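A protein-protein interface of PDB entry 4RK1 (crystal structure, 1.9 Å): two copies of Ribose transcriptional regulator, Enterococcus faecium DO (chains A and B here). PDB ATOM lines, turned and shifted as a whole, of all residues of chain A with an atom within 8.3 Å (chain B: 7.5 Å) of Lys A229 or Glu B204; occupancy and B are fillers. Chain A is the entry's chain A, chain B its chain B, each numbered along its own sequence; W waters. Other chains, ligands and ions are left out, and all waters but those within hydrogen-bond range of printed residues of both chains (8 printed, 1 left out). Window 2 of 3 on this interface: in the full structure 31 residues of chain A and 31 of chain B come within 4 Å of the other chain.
The guanidinium group (NH2) of Arg B201 is in salt-bridge range of the side-chain carboxylate (OE1) of Glu A226. The side-chain hydroxyl (OH) of Tyr A227 is in hydrogen-bond range of the guanidinium group (NH1) of Arg B201 (3.5 Å). The side-chain amino group of Lys A231 is in salt-bridge range of the side-chain carboxylate of Glu B205, at 2.8 Å.
Of the 19 printed residues of chain B, 8 touch a printed residue of chain A. Printed residues of chain B that touch a printed residue of chain A: Phe B197, Gly B198, Arg B201, Glu B204, Glu B205, Tyr B227, Ile B228 and Lys B229. Hydrophobic or aromatic side chains of chain B that line the printed part of chain A: Tyr B227 and Ile B228. Of the 17 printed residues of chain A, 7 touch a printed residue of chain B. Printed residues of chain A that touch a printed residue of chain B: Phe A197, Glu A204, Met A224, Glu A226, Tyr A227, Lys A229 and Lys A231. Hydrophobic or aromatic side chains of chain A that line the printed part of chain B: Met A224 and Tyr A227. Among the printed residues, 11 pairs touch across the chains.
Tyr B227 touches Phe A197 (CD2 to O, 3.5 Å). Tyr B227 touches Glu A204. Glu A204 touches Lys B229. CE of Met A224 touches CG2 of Ile B228 (3.7 Å). O of Phe B197 touches CD2 of Tyr A227, at 3.6 Å. Tyr A227 touches Gly B198 (CE2 to CA, 3.8 Å). OE1 of Glu B204 touches O of Tyr A227, 3.9 Å away. CD of Lys A229 touches CG of Glu B204 (3.8 Å).
Of the printed residues of chain B, Lys A229 touches Glu B204. Glu B204 touches two residues of chain A. Of the printed residues of chain A, Arg B201 touches Glu A226 (3.2 Å) and Tyr A227 (3.5 Å). Printed residues of chain A within 4 Å of Ile B228: Met A224. The nearest residue of chain B that does not touch Lys A229 is Lys B208 (5.3 Å).
Water W8 lies within hydrogen-bond range of the side-chain carboxylate of Glu A204 (2.6 Å) and the backbone carbonyl oxygen of Tyr B227 (2.6 Å). Water W6 lies within hydrogen-bond range of the backbone carbonyl oxygen of Tyr A227 and the side-chain carboxylate of Glu B204. Water W7 lies within hydrogen-bond range of O of Glu B204, O of Lys B208 and NZ of Lys A229. Water W2 lies within hydrogen-bond range of NZ of Lys B229 (2.8 Å) and O of Glu A204 (2.9 Å). Water W1 lies within hydrogen-bond range of the backbone carbonyl oxygen of Lys A229 (3.0 Å) and the backbone carbonyl oxygen of Lys B229 (3.5 Å). Water W5 lies within hydrogen-bond range of NZ of Lys B229 (3.3 Å) and O of Glu A204 (3.5 Å).
Phe A197 touches Tyr B227, and with the chains exchanged Tyr A227 touches Phe B197. Glu A204 touches Tyr B227, and with the chains exchanged Tyr A227 touches Glu B204. Glu A204 touches Lys B229, and with the chains exchanged Lys A229 touches Glu B204. Positions printed for both chains: 197, 200, 204, 209, 210, 227, 228, 229 and 230. Of the 11 pairs that touch across the chains among the printed residues, 6 have their exchanged pair printed and touching as well.
The backbone carbonyl oxygen (O) of Lys A231 lies within hydrogen-bond range of the backbone NH (N) of Phe A274. The backbone carbonyl oxygen (O) of Lys A231 is in hydrogen-bond range of the backbone NH (N) of Ser A275, at 3.4 Å. The guanidinium group (NE) of Arg B201 lies within salt-bridge range of the side-chain carboxylate (OE2) of Glu B205 (3.0 Å).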
ATOM      1  N   PHE A 197     -29.523  16.233  -3.136  1.00  0.00           N
ATOM      2  CA  PHE A 197     -28.385  15.657  -3.845  1.00  0.00           C
ATOM      3  C   PHE A 197     -28.029  16.457  -5.101  1.00  0.00           C
ATOM      4  O   PHE A 197     -26.855  16.597  -5.429  1.00  0.00           O
ATOM      5  CB  PHE A 197     -28.643  14.213  -4.256  1.00  0.00           C
ATOM      6  CG  PHE A 197     -28.958  13.287  -3.115  1.00  0.00           C
ATOM      7  CD1 PHE A 197     -28.596  13.587  -1.804  1.00  0.00           C
ATOM      8  CD2 PHE A 197     -29.595  12.078  -3.371  1.00  0.00           C
ATOM      9  CE1 PHE A 197     -28.904  12.707  -0.769  1.00  0.00           C
ATOM     10  CE2 PHE A 197     -29.878  11.193  -2.346  1.00  0.00           C
ATOM     11  CZ  PHE A 197     -29.539  11.512  -1.045  1.00  0.00           C
ATOM     12  N   TYR A 200     -26.049  19.382  -3.909  1.00  0.00           N
ATOM     13  CA  TYR A 200     -24.675  18.974  -3.655  1.00  0.00           C
ATOM     14  C   TYR A 200     -23.841  19.014  -4.930  1.00  0.00           C
ATOM     15  O   TYR A 200     -22.777  19.593  -4.942  1.00  0.00           O
ATOM     16  CB  TYR A 200     -24.585  17.560  -3.111  1.00  0.00           C
ATOM     17  CG  TYR A 200     -24.716  17.410  -1.617  1.00  0.00           C
ATOM     18  CD1 TYR A 200     -25.770  17.989  -0.916  1.00  0.00           C
ATOM     19  CD2 TYR A 200     -23.809  16.627  -0.909  1.00  0.00           C
ATOM     20  CE1 TYR A 200     -25.903  17.813   0.456  1.00  0.00           C
ATOM     21  CE2 TYR A 200     -23.931  16.445   0.458  1.00  0.00           C
ATOM     22  CZ  TYR A 200     -24.985  17.028   1.133  1.00  0.00           C
ATOM     23  OH  TYR A 200     -25.095  16.838   2.478  1.00  0.00           O
ATOM     24  N   GLU A 204     -20.856  21.676  -5.560  1.00  0.00           N
ATOM     25  CA  GLU A 204     -19.512  21.128  -5.763  1.00  0.00           C
ATOM     26  C   GLU A 204     -18.875  21.661  -7.058  1.00  0.00           C
ATOM     27  O   GLU A 204     -17.737  22.134  -7.051  1.00  0.00           O
ATOM     28  CB  GLU A 204     -19.558  19.611  -5.762  1.00  0.00           C
ATOM     29  CG  GLU A 204     -19.867  19.035  -4.391  1.00  0.00           C
ATOM     30  CD  GLU A 204     -20.467  17.631  -4.411  1.00  0.00           C
ATOM     31  OE1 GLU A 204     -20.676  17.044  -5.500  1.00  0.00           O
ATOM     32  OE2 GLU A 204     -20.735  17.111  -3.302  1.00  0.00           O
ATOM     33  N   SER A 209     -18.725  24.778  -0.775  1.00  0.00           N
ATOM     34  CA  SER A 209     -18.611  23.717   0.223  1.00  0.00           C
ATOM     35  C   SER A 209     -19.855  23.703   1.082  1.00  0.00           C
ATOM     36  O   SER A 209     -20.517  24.728   1.267  1.00  0.00           O
ATOM     37  CB  SER A 209     -17.381  23.936   1.113  1.00  0.00           C
ATOM     38  OG  SER A 209     -16.193  23.669   0.402  1.00  0.00           O
ATOM     39  N   ILE A 210     -20.160  22.522   1.602  1.00  0.00           N
ATOM     40  CA  ILE A 210     -21.286  22.302   2.491  1.00  0.00           C
ATOM     41  C   ILE A 210     -20.692  21.703   3.770  1.00  0.00           C
ATOM     42  O   ILE A 210     -20.002  20.687   3.685  1.00  0.00           O
ATOM     43  CB  ILE A 210     -22.268  21.285   1.874  1.00  0.00           C
ATOM     44  CG1 ILE A 210     -22.788  21.796   0.529  1.00  0.00           C
ATOM     45  CG2 ILE A 210     -23.431  20.998   2.828  1.00  0.00           C
ATOM     46  CD1 ILE A 210     -23.368  20.707  -0.347  1.00  0.00           C
ATOM     47  N   PRO A 211     -20.942  22.286   4.948  1.00  0.00           N
ATOM     48  CA  PRO A 211     -21.872  23.387   5.163  1.00  0.00           C
ATOM     49  C   PRO A 211     -21.258  24.791   5.174  1.00  0.00           C
ATOM     50  O   PRO A 211     -21.964  25.757   5.486  1.00  0.00           O
ATOM     51  CB  PRO A 211     -22.409  23.073   6.555  1.00  0.00           C
ATOM     52  CG  PRO A 211     -21.211  22.517   7.263  1.00  0.00           C
ATOM     53  CD  PRO A 211     -20.433  21.751   6.229  1.00  0.00           C
ATOM     54  N   MET A 224     -29.344   6.800   0.896  1.00  0.00           N
ATOM     55  CA  MET A 224     -28.217   7.535   0.296  1.00  0.00           C
ATOM     56  C   MET A 224     -27.723   8.690   1.132  1.00  0.00           C
ATOM     57  O   MET A 224     -26.566   9.108   0.968  1.00  0.00           O
ATOM     58  CB  MET A 224     -28.607   7.962  -1.142  1.00  0.00           C
ATOM     59  CG  MET A 224     -27.447   8.459  -2.009  1.00  0.00           C
ATOM     60  SD  MET A 224     -26.270   6.949  -2.521  1.00  0.00           S
ATOM     61  CE  MET A 224     -24.576   7.921  -2.801  1.00  0.00           C
ATOM     62  N   CYS A 225     -28.563   9.231   2.025  1.00  0.00           N
ATOM     63  CA  CYS A 225     -28.134  10.335   2.928  1.00  0.00           C
ATOM     64  C   CYS A 225     -26.862  10.004   3.704  1.00  0.00           C
ATOM     65  O   CYS A 225     -26.070  10.889   4.018  1.00  0.00           O
ATOM     66  CB  CYS A 225     -29.218  10.691   3.936  1.00  0.00           C
ATOM     67  SG  CYS A 225     -30.714  11.416   3.235  1.00  0.00           S
ATOM     68  N   GLU A 226     -26.674   8.722   3.998  1.00  0.00           N
ATOM     69  CA  GLU A 226     -25.513   8.268   4.760  1.00  0.00           C
ATOM     70  C   GLU A 226     -24.294   7.919   3.910  1.00  0.00           C
ATOM     71  O   GLU A 226     -23.248   7.597   4.464  1.00  0.00           O
ATOM     72  CB  GLU A 226     -25.918   7.079   5.637  1.00  0.00           C
ATOM     73  CG  GLU A 226     -26.902   7.507   6.710  1.00  0.00           C
ATOM     74  CD  GLU A 226     -27.085   6.495   7.815  1.00  0.00           C
ATOM     75  OE1 GLU A 226     -27.090   5.283   7.525  1.00  0.00           O
ATOM     76  OE2 GLU A 226     -27.238   6.925   8.974  1.00  0.00           O
ATOM     77  N   TYR A 227     -24.425   8.004   2.580  1.00  0.00           N
ATOM     78  CA  TYR A 227     -23.364   7.642   1.654  1.00  0.00           C
ATOM     79  C   TYR A 227     -22.760   8.830   0.932  1.00  0.00           C
ATOM     80  O   TYR A 227     -21.760   8.686   0.257  1.00  0.00           O
ATOM     81  CB  TYR A 227     -23.880   6.621   0.643  1.00  0.00           C
ATOM     82  CG  TYR A 227     -24.212   5.303   1.291  1.00  0.00           C
ATOM     83  CD1 TYR A 227     -25.392   5.127   1.983  1.00  0.00           C
ATOM     84  CD2 TYR A 227     -23.327   4.236   1.219  1.00  0.00           C
ATOM     85  CE1 TYR A 227     -25.696   3.922   2.594  1.00  0.00           C
ATOM     86  CE2 TYR A 227     -23.620   3.035   1.813  1.00  0.00           C
ATOM     87  CZ  TYR A 227     -24.796   2.873   2.499  1.00  0.00           C
ATOM     88  OH  TYR A 227     -25.039   1.647   3.079  1.00  0.00           O
ATOM     89  N   ILE A 228     -23.376   9.996   1.053  1.00  0.00           N
ATOM     90  CA  ILE A 228     -22.768  11.219   0.541  1.00  0.00           C
ATOM     91  C   ILE A 228     -21.995  11.940   1.636  1.00  0.00           C
ATOM     92  O   ILE A 228     -22.096  11.616   2.823  1.00  0.00           O
ATOM     93  CB  ILE A 228     -23.808  12.163  -0.106  1.00  0.00           C
ATOM     94  CG1 ILE A 228     -24.856  12.637   0.915  1.00  0.00           C
ATOM     95  CG2 ILE A 228     -24.462  11.479  -1.293  1.00  0.00           C
ATOM     96  CD1 ILE A 228     -25.832  13.619   0.304  1.00  0.00           C
ATOM     97  N   LYS A 229     -21.221  12.932   1.221  1.00  0.00           N
ATOM     98  CA  LYS A 229     -20.312  13.624   2.118  1.00  0.00           C
ATOM     99  C   LYS A 229     -20.377  15.120   1.835  1.00  0.00           C
ATOM    100  O   LYS A 229     -20.163  15.521   0.700  1.00  0.00           O
ATOM    101  CB  LYS A 229     -18.891  13.093   1.899  1.00  0.00           C
ATOM    102  CG  LYS A 229     -17.802  13.902   2.578  1.00  0.00           C
ATOM    103  CD  LYS A 229     -16.458  13.196   2.492  1.00  0.00           C
ATOM    104  CE  LYS A 229     -15.321  14.107   2.935  1.00  0.00           C
ATOM    105  NZ  LYS A 229     -14.100  13.323   3.274  1.00  0.00           N
ATOM    106  N   PRO A 230     -20.686  15.945   2.832  1.00  0.00           N
ATOM    107  CA  PRO A 230     -21.060  15.503   4.168  1.00  0.00           C
ATOM    108  C   PRO A 230     -22.400  14.782   4.184  1.00  0.00           C
ATOM    109  O   PRO A 230     -23.263  15.024   3.328  1.00  0.00           O
ATOM    110  CB  PRO A 230     -21.192  16.818   4.924  1.00  0.00           C
ATOM    111  CG  PRO A 230     -21.713  17.762   3.886  1.00  0.00           C
ATOM    112  CD  PRO A 230     -20.973  17.382   2.636  1.00  0.00           C
ATOM    113  N   LYS A 231     -22.577  13.911   5.166  1.00  0.00           N
ATOM    114  CA  LYS A 231     -23.825  13.193   5.304  1.00  0.00           C
ATOM    115  C   LYS A 231     -24.964  14.188   5.519  1.00  0.00           C
ATOM    116  O   LYS A 231     -24.817  15.172   6.243  1.00  0.00           O
ATOM    117  CB  LYS A 231     -23.763  12.210   6.466  1.00  0.00           C
ATOM    118  CG  LYS A 231     -22.846  11.010   6.252  1.00  0.00           C
ATOM    119  CD  LYS A 231     -22.736  10.241   7.569  1.00  0.00           C
ATOM    120  CE  LYS A 231     -22.197   8.828   7.432  1.00  0.00           C
ATOM    121  NZ  LYS A 231     -20.820   8.789   6.901  1.00  0.00           N
ATOM    122  N   LEU A 232     -26.098  13.899   4.899  1.00  0.00           N
ATOM    123  CA  LEU A 232     -27.196  14.853   4.805  1.00  0.00           C
ATOM    124  C   LEU A 232     -28.088  14.859   6.040  1.00  0.00           C
ATOM    125  O   LEU A 232     -28.635  13.845   6.448  1.00  0.00           O
ATOM    126  CB  LEU A 232     -28.036  14.566   3.555  1.00  0.00           C
ATOM    127  CG  LEU A 232     -29.252  15.460   3.274  1.00  0.00           C
ATOM    128  CD1 LEU A 232     -28.842  16.903   3.087  1.00  0.00           C
ATOM    129  CD2 LEU A 232     -30.000  14.976   2.043  1.00  0.00           C
ATOM    130  N   PHE A 274     -24.384  16.295   9.066  1.00  0.00           N
ATOM    131  CA  PHE A 274     -23.256  17.215   8.939  1.00  0.00           C
ATOM    132  C   PHE A 274     -23.367  18.238   7.810  1.00  0.00           C
ATOM    133  O   PHE A 274     -22.373  18.874   7.448  1.00  0.00           O
ATOM    134  CB  PHE A 274     -21.978  16.381   8.782  1.00  0.00           C
ATOM    135  CG  PHE A 274     -21.632  15.592  10.011  1.00  0.00           C
ATOM    136  CD1 PHE A 274     -20.915  16.185  11.045  1.00  0.00           C
ATOM    137  CD2 PHE A 274     -22.059  14.280  10.161  1.00  0.00           C
ATOM    138  CE1 PHE A 274     -20.610  15.468  12.196  1.00  0.00           C
ATOM    139  CE2 PHE A 274     -21.760  13.560  11.310  1.00  0.00           C
ATOM    140  CZ  PHE A 274     -21.033  14.156  12.326  1.00  0.00           C
ATOM    141  N   SER A 275     -24.565  18.419   7.272  1.00  0.00           N
ATOM    142  CA  SER A 275     -24.775  19.339   6.139  1.00  0.00           C
ATOM    143  C   SER A 275     -25.308  20.692   6.581  1.00  0.00           C
ATOM    144  O   SER A 275     -25.653  21.518   5.732  1.00  0.00           O
ATOM    145  CB  SER A 275     -25.744  18.717   5.125  1.00  0.00           C
ATOM    146  OG  SER A 275     -27.026  18.500   5.708  1.00  0.00           O
ATOM    147  N   THR B 177     -15.341  -2.790   3.479  1.00  0.00           N
ATOM    148  CA  THR B 177     -14.300  -1.773   3.545  1.00  0.00           C
ATOM    149  C   THR B 177     -13.132  -2.149   4.456  1.00  0.00           C
ATOM    150  O   THR B 177     -11.984  -1.900   4.109  1.00  0.00           O
ATOM    151  CB  THR B 177     -14.854  -0.419   4.038  1.00  0.00           C
ATOM    152  OG1 THR B 177     -15.950  -0.007   3.213  1.00  0.00           O
ATOM    153  CG2 THR B 177     -13.767   0.640   3.992  1.00  0.00           C
ATOM    154  N   PHE B 197     -20.598   2.919  -4.141  1.00  0.00           N
ATOM    155  CA  PHE B 197     -21.064   3.959  -3.210  1.00  0.00           C
ATOM    156  C   PHE B 197     -20.834   3.513  -1.755  1.00  0.00           C
ATOM    157  O   PHE B 197     -20.441   4.308  -0.909  1.00  0.00           O
ATOM    158  CB  PHE B 197     -22.540   4.280  -3.391  1.00  0.00           C
ATOM    159  CG  PHE B 197     -22.924   4.747  -4.776  1.00  0.00           C
ATOM    160  CD1 PHE B 197     -21.989   5.261  -5.659  1.00  0.00           C
ATOM    161  CD2 PHE B 197     -24.251   4.664  -5.186  1.00  0.00           C
ATOM    162  CE1 PHE B 197     -22.365   5.681  -6.918  1.00  0.00           C
ATOM    163  CE2 PHE B 197     -24.631   5.085  -6.442  1.00  0.00           C
ATOM    164  CZ  PHE B 197     -23.689   5.594  -7.312  1.00  0.00           C
ATOM    165  N   GLY B 198     -21.090   2.239  -1.486  1.00  0.00           N
ATOM    166  CA  GLY B 198     -20.761   1.631  -0.195  1.00  0.00           C
ATOM    167  C   GLY B 198     -19.316   1.812   0.205  1.00  0.00           C
ATOM    168  O   GLY B 198     -19.023   2.172   1.349  1.00  0.00           O
ATOM    169  N   LEU B 199     -18.414   1.589  -0.747  1.00  0.00           N
ATOM    170  CA  LEU B 199     -16.989   1.792  -0.528  1.00  0.00           C
ATOM    171  C   LEU B 199     -16.649   3.239  -0.254  1.00  0.00           C
ATOM    172  O   LEU B 199     -15.831   3.527   0.617  1.00  0.00           O
ATOM    173  CB  LEU B 199     -16.170   1.304  -1.720  1.00  0.00           C
ATOM    174  CG  LEU B 199     -16.007  -0.205  -1.859  1.00  0.00           C
ATOM    175  CD1 LEU B 199     -15.340  -0.507  -3.193  1.00  0.00           C
ATOM    176  CD2 LEU B 199     -15.194  -0.772  -0.707  1.00  0.00           C
ATOM    177  N   TYR B 200     -17.256   4.157  -0.997  1.00  0.00           N
ATOM    178  CA  TYR B 200     -17.030   5.567  -0.726  1.00  0.00           C
ATOM    179  C   TYR B 200     -17.312   5.867   0.739  1.00  0.00           C
ATOM    180  O   TYR B 200     -16.523   6.530   1.400  1.00  0.00           O
ATOM    181  CB  TYR B 200     -17.929   6.458  -1.574  1.00  0.00           C
ATOM    182  CG  TYR B 200     -17.415   6.868  -2.938  1.00  0.00           C
ATOM    183  CD1 TYR B 200     -16.935   5.939  -3.851  1.00  0.00           C
ATOM    184  CD2 TYR B 200     -17.492   8.199  -3.343  1.00  0.00           C
ATOM    185  CE1 TYR B 200     -16.508   6.326  -5.114  1.00  0.00           C
ATOM    186  CE2 TYR B 200     -17.083   8.592  -4.599  1.00  0.00           C
ATOM    187  CZ  TYR B 200     -16.602   7.655  -5.488  1.00  0.00           C
ATOM    188  OH  TYR B 200     -16.193   8.061  -6.736  1.00  0.00           O
ATOM    189  N   ARG B 201     -18.454   5.396   1.232  1.00  0.00           N
ATOM    190  CA  ARG B 201     -18.846   5.666   2.598  1.00  0.00           C
ATOM    191  C   ARG B 201     -17.837   5.071   3.577  1.00  0.00           C
ATOM    192  O   ARG B 201     -17.368   5.759   4.476  1.00  0.00           O
ATOM    193  CB  ARG B 201     -20.242   5.121   2.888  1.00  0.00           C
ATOM    194  CG  ARG B 201     -20.689   5.373   4.322  1.00  0.00           C
ATOM    195  CD  ARG B 201     -21.986   4.655   4.641  1.00  0.00           C
ATOM    196  NE  ARG B 201     -22.301   4.741   6.058  1.00  0.00           N
ATOM    197  CZ  ARG B 201     -23.354   4.166   6.636  1.00  0.00           C
ATOM    198  NH1 ARG B 201     -24.214   3.456   5.922  1.00  0.00           N
ATOM    199  NH2 ARG B 201     -23.541   4.303   7.943  1.00  0.00           N
ATOM    200  N   GLY B 202     -17.512   3.796   3.398  1.00  0.00           N
ATOM    201  CA  GLY B 202     -16.542   3.131   4.254  1.00  0.00           C
ATOM    202  C   GLY B 202     -15.199   3.833   4.275  1.00  0.00           C
ATOM    203  O   GLY B 202     -14.609   4.030   5.336  1.00  0.00           O
ATOM    204  N   LEU B 203     -14.713   4.241   3.110  1.00  0.00           N
ATOM    205  CA  LEU B 203     -13.396   4.880   3.031  1.00  0.00           C
ATOM    206  C   LEU B 203     -13.393   6.267   3.640  1.00  0.00           C
ATOM    207  O   LEU B 203     -12.451   6.641   4.355  1.00  0.00           O
ATOM    208  CB  LEU B 203     -12.899   4.931   1.585  1.00  0.00           C
ATOM    209  CG  LEU B 203     -12.571   3.549   1.032  1.00  0.00           C
ATOM    210  CD1 LEU B 203     -12.346   3.629  -0.464  1.00  0.00           C
ATOM    211  CD2 LEU B 203     -11.362   2.948   1.739  1.00  0.00           C
ATOM    212  N   GLU B 204     -14.452   7.029   3.372  1.00  0.00           N
ATOM    213  CA  GLU B 204     -14.635   8.332   4.015  1.00  0.00           C
ATOM    214  C   GLU B 204     -14.601   8.219   5.549  1.00  0.00           C
ATOM    215  O   GLU B 204     -13.902   8.981   6.219  1.00  0.00           O
ATOM    216  CB  GLU B 204     -15.947   8.969   3.552  1.00  0.00           C
ATOM    217  CG  GLU B 204     -15.907   9.416   2.092  1.00  0.00           C
ATOM    218  CD  GLU B 204     -17.275   9.498   1.417  1.00  0.00           C
ATOM    219  OE1 GLU B 204     -18.314   9.206   2.055  1.00  0.00           O
ATOM    220  OE2 GLU B 204     -17.303   9.867   0.221  1.00  0.00           O
ATOM    221  N   GLU B 205     -15.335   7.255   6.090  1.00  0.00           N
ATOM    222  CA  GLU B 205     -15.395   7.063   7.540  1.00  0.00           C
ATOM    223  C   GLU B 205     -14.061   6.623   8.148  1.00  0.00           C
ATOM    224  O   GLU B 205     -13.779   6.931   9.306  1.00  0.00           O
ATOM    225  CB  GLU B 205     -16.513   6.089   7.900  1.00  0.00           C
ATOM    226  CG  GLU B 205     -17.884   6.703   7.633  1.00  0.00           C
ATOM    227  CD  GLU B 205     -19.038   5.791   7.951  1.00  0.00           C
ATOM    228  OE1 GLU B 205     -18.805   4.711   8.539  1.00  0.00           O
ATOM    229  OE2 GLU B 205     -20.182   6.177   7.604  1.00  0.00           O
ATOM    230  N   ALA B 206     -13.237   5.936   7.361  1.00  0.00           N
ATOM    231  CA  ALA B 206     -11.897   5.528   7.794  1.00  0.00           C
ATOM    232  C   ALA B 206     -10.837   6.610   7.566  1.00  0.00           C
ATOM    233  O   ALA B 206      -9.662   6.385   7.823  1.00  0.00           O
ATOM    234  CB  ALA B 206     -11.491   4.242   7.092  1.00  0.00           C
ATOM    235  N   GLY B 207     -11.244   7.782   7.085  1.00  0.00           N
ATOM    236  CA  GLY B 207     -10.315   8.884   6.871  1.00  0.00           C
ATOM    237  C   GLY B 207      -9.502   8.754   5.596  1.00  0.00           C
ATOM    238  O   GLY B 207      -8.485   9.420   5.440  1.00  0.00           O
ATOM    239  N   LYS B 208      -9.953   7.912   4.671  1.00  0.00           N
ATOM    240  CA  LYS B 208      -9.245   7.723   3.414  1.00  0.00           C
ATOM    241  C   LYS B 208      -9.859   8.616   2.335  1.00  0.00           C
ATOM    242  O   LYS B 208     -10.946   9.161   2.520  1.00  0.00           O
ATOM    243  CB  LYS B 208      -9.278   6.259   3.006  1.00  0.00           C
ATOM    244  CG  LYS B 208      -8.674   5.305   4.025  1.00  0.00           C
ATOM    245  CD  LYS B 208      -7.204   5.591   4.292  1.00  0.00           C
ATOM    246  CE  LYS B 208      -6.633   4.623   5.313  1.00  0.00           C
ATOM    247  NZ  LYS B 208      -5.168   4.826   5.460  1.00  0.00           N
ATOM    248  N   SER B 209      -9.132   8.780   1.233  1.00  0.00           N
ATOM    249  CA  SER B 209      -9.536   9.657   0.126  1.00  0.00           C
ATOM    250  C   SER B 209      -9.546   8.894  -1.191  1.00  0.00           C
ATOM    251  O   SER B 209      -8.760   7.968  -1.391  1.00  0.00           O
ATOM    252  CB  SER B 209      -8.577  10.842  -0.006  1.00  0.00           C
ATOM    253  OG  SER B 209      -8.712  11.740   1.072  1.00  0.00           O
ATOM    254  N   ILE B 210     -10.437   9.304  -2.092  1.00  0.00           N
ATOM    255  CA  ILE B 210     -10.526   8.728  -3.435  1.00  0.00           C
ATOM    256  C   ILE B 210     -10.239   9.875  -4.402  1.00  0.00           C
ATOM    257  O   ILE B 210     -10.868  10.928  -4.283  1.00  0.00           O
ATOM    258  CB  ILE B 210     -11.927   8.130  -3.669  1.00  0.00           C
ATOM    259  CG1 ILE B 210     -12.203   7.024  -2.645  1.00  0.00           C
ATOM    260  CG2 ILE B 210     -12.069   7.568  -5.080  1.00  0.00           C
ATOM    261  CD1 ILE B 210     -13.673   6.773  -2.410  1.00  0.00           C
ATOM    262  N   TYR B 227     -23.361  12.651  -9.019  1.00  0.00           N
ATOM    263  CA  TYR B 227     -23.752  13.456  -7.881  1.00  0.00           C
ATOM    264  C   TYR B 227     -22.875  13.223  -6.662  1.00  0.00           C
ATOM    265  O   TYR B 227     -22.938  13.986  -5.718  1.00  0.00           O
ATOM    266  CB  TYR B 227     -25.236  13.224  -7.545  1.00  0.00           C
ATOM    267  CG  TYR B 227     -26.146  13.737  -8.636  1.00  0.00           C
ATOM    268  CD1 TYR B 227     -26.364  12.997  -9.787  1.00  0.00           C
ATOM    269  CD2 TYR B 227     -26.764  14.984  -8.533  1.00  0.00           C
ATOM    270  CE1 TYR B 227     -27.172  13.469 -10.809  1.00  0.00           C
ATOM    271  CE2 TYR B 227     -27.567  15.462  -9.551  1.00  0.00           C
ATOM    272  CZ  TYR B 227     -27.774  14.705 -10.680  1.00  0.00           C
ATOM    273  OH  TYR B 227     -28.584  15.199 -11.686  1.00  0.00           O
ATOM    274  N   ILE B 228     -22.075  12.164  -6.664  1.00  0.00           N
ATOM    275  CA  ILE B 228     -21.101  11.973  -5.595  1.00  0.00           C
ATOM    276  C   ILE B 228     -19.783  12.644  -5.947  1.00  0.00           C
ATOM    277  O   ILE B 228     -19.572  13.065  -7.082  1.00  0.00           O
ATOM    278  CB  ILE B 228     -20.866  10.484  -5.266  1.00  0.00           C
ATOM    279  CG1 ILE B 228     -20.363   9.714  -6.499  1.00  0.00           C
ATOM    280  CG2 ILE B 228     -22.133   9.881  -4.696  1.00  0.00           C
ATOM    281  CD1 ILE B 228     -20.086   8.260  -6.215  1.00  0.00           C
ATOM    282  N   LYS B 229     -18.898  12.730  -4.961  1.00  0.00           N
ATOM    283  CA  LYS B 229     -17.619  13.421  -5.123  1.00  0.00           C
ATOM    284  C   LYS B 229     -16.517  12.565  -4.498  1.00  0.00           C
ATOM    285  O   LYS B 229     -16.613  12.204  -3.337  1.00  0.00           O
ATOM    286  CB  LYS B 229     -17.686  14.806  -4.464  1.00  0.00           C
ATOM    287  CG  LYS B 229     -16.422  15.633  -4.596  1.00  0.00           C
ATOM    288  CD  LYS B 229     -16.672  17.071  -4.178  1.00  0.00           C
ATOM    289  CE  LYS B 229     -15.375  17.813  -3.895  1.00  0.00           C
ATOM    290  NZ  LYS B 229     -15.593  19.287  -3.845  1.00  0.00           N
ATOM    291  N   PRO B 230     -15.496  12.193  -5.265  1.00  0.00           N
ATOM    292  CA  PRO B 230     -15.389  12.506  -6.684  1.00  0.00           C
ATOM    293  C   PRO B 230     -16.418  11.731  -7.514  1.00  0.00           C
ATOM    294  O   PRO B 230     -16.864  10.648  -7.105  1.00  0.00           O
ATOM    295  CB  PRO B 230     -13.974  12.022  -7.022  1.00  0.00           C
ATOM    296  CG  PRO B 230     -13.765  10.869  -6.099  1.00  0.00           C
ATOM    297  CD  PRO B 230     -14.441  11.261  -4.823  1.00  0.00           C
HETATM  298  O   HOH W   1     -18.010  14.486  -1.086  1.00  0.00           O
HETATM  299  O   HOH W   2     -16.057  21.957  -4.724  1.00  0.00           O
HETATM  300  O   HOH W   3     -12.918  11.123   1.921  1.00  0.00           O
HETATM  301  O   HOH W   4     -20.139  15.543  -7.931  1.00  0.00           O
HETATM  302  O   HOH W   5     -16.139  19.041  -7.082  1.00  0.00           O
HETATM  303  O   HOH W   6     -19.686   9.816  -0.888  1.00  0.00           O
HETATM  304  O   HOH W   7     -12.281  10.886   4.956  1.00  0.00           O
HETATM  305  O   HOH W   8     -21.918  14.778  -3.427  1.00  0.00           O
